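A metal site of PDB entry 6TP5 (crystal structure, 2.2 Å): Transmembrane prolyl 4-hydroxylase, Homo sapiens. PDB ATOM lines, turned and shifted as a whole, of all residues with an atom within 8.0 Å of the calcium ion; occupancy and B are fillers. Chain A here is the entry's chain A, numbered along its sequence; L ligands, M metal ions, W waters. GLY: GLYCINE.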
ATOM      1  N   HIS A 123     -16.205  12.573 -25.461  1.00  0.00           N
ATOM      2  CA  HIS A 123     -16.622  11.186 -25.442  1.00  0.00           C
ATOM      3  C   HIS A 123     -18.072  11.097 -25.888  1.00  0.00           C
ATOM      4  O   HIS A 123     -18.900  11.916 -25.469  1.00  0.00           O
ATOM      5  CB  HIS A 123     -16.474  10.582 -24.036  1.00  0.00           C
ATOM      6  CG  HIS A 123     -15.060  10.439 -23.565  1.00  0.00           C
ATOM      7  ND1 HIS A 123     -14.290  11.513 -23.187  1.00  0.00           N
ATOM      8  CD2 HIS A 123     -14.285   9.342 -23.402  1.00  0.00           C
ATOM      9  CE1 HIS A 123     -13.095  11.091 -22.810  1.00  0.00           C
ATOM     10  NE2 HIS A 123     -13.067   9.778 -22.937  1.00  0.00           N
ATOM     11  N   LEU A 124     -18.369  10.112 -26.732  1.00  0.00           N
ATOM     12  CA  LEU A 124     -19.746   9.843 -27.149  1.00  0.00           C
ATOM     13  C   LEU A 124     -20.352   8.833 -26.186  1.00  0.00           C
ATOM     14  O   LEU A 124     -20.045   7.635 -26.250  1.00  0.00           O
ATOM     15  CB  LEU A 124     -19.794   9.327 -28.587  1.00  0.00           C
ATOM     16  CG  LEU A 124     -19.295  10.292 -29.666  1.00  0.00           C
ATOM     17  CD1 LEU A 124     -19.712   9.829 -31.058  1.00  0.00           C
ATOM     18  CD2 LEU A 124     -19.792  11.707 -29.391  1.00  0.00           C
ATOM     19  N   TYR A 150     -21.025  -1.885 -32.278  1.00  0.00           N
ATOM     20  CA  TYR A 150     -19.656  -1.611 -31.841  1.00  0.00           C
ATOM     21  C   TYR A 150     -18.811  -2.881 -31.858  1.00  0.00           C
ATOM     22  O   TYR A 150     -17.689  -2.882 -32.377  1.00  0.00           O
ATOM     23  CB  TYR A 150     -19.636  -1.017 -30.428  1.00  0.00           C
ATOM     24  CG  TYR A 150     -20.081   0.420 -30.301  1.00  0.00           C
ATOM     25  CD1 TYR A 150     -20.345   1.200 -31.417  1.00  0.00           C
ATOM     26  CD2 TYR A 150     -20.247   0.999 -29.042  1.00  0.00           C
ATOM     27  CE1 TYR A 150     -20.757   2.519 -31.297  1.00  0.00           C
ATOM     28  CE2 TYR A 150     -20.665   2.309 -28.903  1.00  0.00           C
ATOM     29  CZ  TYR A 150     -20.920   3.069 -30.031  1.00  0.00           C
ATOM     30  OH  TYR A 150     -21.338   4.366 -29.892  1.00  0.00           O
ATOM     31  N   ALA A 155     -15.431  -1.225 -32.852  1.00  0.00           N
ATOM     32  CA  ALA A 155     -15.309   0.203 -32.624  1.00  0.00           C
ATOM     33  C   ALA A 155     -14.976   0.562 -31.180  1.00  0.00           C
ATOM     34  O   ALA A 155     -14.491   1.674 -30.925  1.00  0.00           O
ATOM     35  CB  ALA A 155     -16.602   0.916 -33.024  1.00  0.00           C
ATOM     36  N   ASP A 156     -15.230  -0.336 -30.222  1.00  0.00           N
ATOM     37  CA  ASP A 156     -15.118  -0.041 -28.797  1.00  0.00           C
ATOM     38  C   ASP A 156     -14.146  -1.028 -28.162  1.00  0.00           C
ATOM     39  O   ASP A 156     -14.572  -1.980 -27.492  1.00  0.00           O
ATOM     40  CB  ASP A 156     -16.475  -0.081 -28.106  1.00  0.00           C
ATOM     41  CG  ASP A 156     -16.409   0.396 -26.679  1.00  0.00           C
ATOM     42  OD1 ASP A 156     -15.328   0.871 -26.264  1.00  0.00           O
ATOM     43  OD2 ASP A 156     -17.427   0.294 -25.965  1.00  0.00           O
ATOM     44  N   PRO A 157     -12.842  -0.807 -28.311  1.00  0.00           N
ATOM     45  CA  PRO A 157     -11.872  -1.806 -27.826  1.00  0.00           C
ATOM     46  C   PRO A 157     -11.982  -2.112 -26.345  1.00  0.00           C
ATOM     47  O   PRO A 157     -11.938  -3.286 -25.962  1.00  0.00           O
ATOM     48  CB  PRO A 157     -10.524  -1.162 -28.187  1.00  0.00           C
ATOM     49  CG  PRO A 157     -10.838  -0.223 -29.304  1.00  0.00           C
ATOM     50  CD  PRO A 157     -12.190   0.312 -29.015  1.00  0.00           C
ATOM     51  N   ASP A 158     -12.108  -1.090 -25.498  1.00  0.00           N
ATOM     52  CA  ASP A 158     -12.232  -1.316 -24.062  1.00  0.00           C
ATOM     53  C   ASP A 158     -13.652  -1.672 -23.633  1.00  0.00           C
ATOM     54  O   ASP A 158     -13.877  -1.885 -22.439  1.00  0.00           O
ATOM     55  CB  ASP A 158     -11.736  -0.087 -23.288  1.00  0.00           C
ATOM     56  CG  ASP A 158     -12.427   1.184 -23.709  1.00  0.00           C
ATOM     57  OD1 ASP A 158     -13.230   1.147 -24.660  1.00  0.00           O
ATOM     58  OD2 ASP A 158     -12.152   2.231 -23.092  1.00  0.00           O
ATOM     59  N   GLY A 159     -14.588  -1.730 -24.569  1.00  0.00           N
ATOM     60  CA  GLY A 159     -15.927  -2.217 -24.307  1.00  0.00           C
ATOM     61  C   GLY A 159     -16.658  -1.580 -23.147  1.00  0.00           C
ATOM     62  O   GLY A 159     -17.260  -2.282 -22.324  1.00  0.00           O
ATOM     63  N   ASP A 160     -16.622  -0.252 -23.048  1.00  0.00           N
ATOM     64  CA  ASP A 160     -17.363   0.458 -22.023  1.00  0.00           C
ATOM     65  C   ASP A 160     -18.615   1.148 -22.564  1.00  0.00           C
ATOM     66  O   ASP A 160     -19.304   1.837 -21.800  1.00  0.00           O
ATOM     67  CB  ASP A 160     -16.449   1.490 -21.334  1.00  0.00           C
ATOM     68  CG  ASP A 160     -15.911   2.544 -22.295  1.00  0.00           C
ATOM     69  OD1 ASP A 160     -16.070   2.388 -23.532  1.00  0.00           O
ATOM     70  OD2 ASP A 160     -15.320   3.524 -21.817  1.00  0.00           O
ATOM     71  N   GLY A 161     -18.933   0.973 -23.845  1.00  0.00           N
ATOM     72  CA  GLY A 161     -20.086   1.612 -24.437  1.00  0.00           C
ATOM     73  C   GLY A 161     -19.885   3.053 -24.838  1.00  0.00           C
ATOM     74  O   GLY A 161     -20.800   3.650 -25.418  1.00  0.00           O
ATOM     75  N   VAL A 162     -18.717   3.624 -24.556  1.00  0.00           N
ATOM     76  CA  VAL A 162     -18.385   5.014 -24.867  1.00  0.00           C
ATOM     77  C   VAL A 162     -17.321   5.030 -25.947  1.00  0.00           C
ATOM     78  O   VAL A 162     -16.324   4.301 -25.855  1.00  0.00           O
ATOM     79  CB  VAL A 162     -17.907   5.761 -23.605  1.00  0.00           C
ATOM     80  CG1 VAL A 162     -17.499   7.183 -23.952  1.00  0.00           C
ATOM     81  CG2 VAL A 162     -18.977   5.723 -22.506  1.00  0.00           C
ATOM     82  N   LEU A 163     -17.514   5.861 -26.968  1.00  0.00           N
ATOM     83  CA  LEU A 163     -16.486   6.096 -27.984  1.00  0.00           C
ATOM     84  C   LEU A 163     -15.773   7.403 -27.642  1.00  0.00           C
ATOM     85  O   LEU A 163     -16.362   8.485 -27.752  1.00  0.00           O
ATOM     86  CB  LEU A 163     -17.095   6.171 -29.375  1.00  0.00           C
ATOM     87  CG  LEU A 163     -17.891   4.959 -29.873  1.00  0.00           C
ATOM     88  CD1 LEU A 163     -18.349   5.235 -31.297  1.00  0.00           C
ATOM     89  CD2 LEU A 163     -17.063   3.681 -29.791  1.00  0.00           C
ATOM     90  N   SER A 164     -14.517   7.305 -27.232  1.00  0.00           N
ATOM     91  CA  SER A 164     -13.710   8.496 -27.066  1.00  0.00           C
ATOM     92  C   SER A 164     -13.388   9.085 -28.433  1.00  0.00           C
ATOM     93  O   SER A 164     -13.637   8.482 -29.481  1.00  0.00           O
ATOM     94  CB  SER A 164     -12.421   8.172 -26.309  1.00  0.00           C
ATOM     95  OG  SER A 164     -11.551   7.390 -27.116  1.00  0.00           O
ATOM     96  N   GLU A 167     -11.062   6.680 -30.161  1.00  0.00           N
ATOM     97  CA  GLU A 167     -11.747   5.511 -30.704  1.00  0.00           C
ATOM     98  C   GLU A 167     -12.568   5.888 -31.918  1.00  0.00           C
ATOM     99  O   GLU A 167     -12.614   5.150 -32.911  1.00  0.00           O
ATOM    100  CB  GLU A 167     -12.632   4.880 -29.641  1.00  0.00           C
ATOM    101  CG  GLU A 167     -11.873   4.076 -28.627  1.00  0.00           C
ATOM    102  CD  GLU A 167     -12.735   3.689 -27.447  1.00  0.00           C
ATOM    103  OE1 GLU A 167     -13.700   4.423 -27.147  1.00  0.00           O
ATOM    104  OE2 GLU A 167     -12.461   2.643 -26.830  1.00  0.00           O
ATOM    105  N   PHE A 168     -13.232   7.046 -31.874  1.00  0.00           N
ATOM    106  CA  PHE A 168     -14.058   7.459 -32.996  1.00  0.00           C
ATOM    107  C   PHE A 168     -13.205   7.728 -34.234  1.00  0.00           C
ATOM    108  O   PHE A 168     -13.528   7.241 -35.326  1.00  0.00           O
ATOM    109  CB  PHE A 168     -14.861   8.702 -32.609  1.00  0.00           C
ATOM    110  CG  PHE A 168     -15.873   9.106 -33.645  1.00  0.00           C
ATOM    111  CD1 PHE A 168     -17.107   8.493 -33.701  1.00  0.00           C
ATOM    112  CD2 PHE A 168     -15.571  10.078 -34.576  1.00  0.00           C
ATOM    113  CE1 PHE A 168     -18.039   8.850 -34.658  1.00  0.00           C
ATOM    114  CE2 PHE A 168     -16.490  10.450 -35.533  1.00  0.00           C
ATOM    115  CZ  PHE A 168     -17.724   9.837 -35.579  1.00  0.00           C
HETATM  116  N   GLY L   1     -16.087  11.299 -18.697  1.00  0.00           N
HETATM  117  CA  GLY L   1     -14.967  10.383 -18.826  1.00  0.00           C
HETATM  118  C   GLY L   1     -15.401   8.976 -19.179  1.00  0.00           C
HETATM  119  O   GLY L   1     -14.579   8.132 -19.549  1.00  0.00           O
HETATM  120  OXT GLY L   1     -16.578   8.630 -19.106  1.00  0.00           O
HETATM  121 CA    CA M   1     -14.497   2.881 -25.392  1.00  0.00          CA
HETATM  122  O   HOH W   1     -13.913   4.644 -23.939  1.00  0.00           O
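Water W1 lies within hydrogen-bond range of OD2 of Asp 160 (2.8 Å) and OD2 of Asp 158 (3.1 Å).
The calcium ion is bound by the side-chain carboxylate (OD1) of Asp 158 (2.3 Å), the side-chain carboxylate (OD1) of Asp 156 (2.3 Å), water W1 (2.4 Å), the backbone carbonyl oxygen (O) of Val 162 (2.4 Å), the side-chain carboxylate (OE1) of Glu 167 (2.5 Å), the side-chain carboxylate (OD1) of Asp 160 (2.5 Å) and the side-chain carboxylate (OE2) of Glu 167 (2.5 Å).
Of the 15 residues printed, 5 come within 4 Å of the calcium ion.
The nearest printed residue that does not touch the calcium ion is Leu 163 (4.5 Å).
The side-chain carboxylate of Asp 156 lies close to the backbone NH of Gly 159 (3.2 Å).
The backbone NH (N) of Gly 161 is in hydrogen-bond range of the side-chain carboxylate (OD2) of Asp 156, 2.7 Å away.
The backbone NH (N) of Glu 167 sits at hydrogen-bond distance from the side-chain hydroxyl (OG) of Ser 164, 3.2 Å away.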
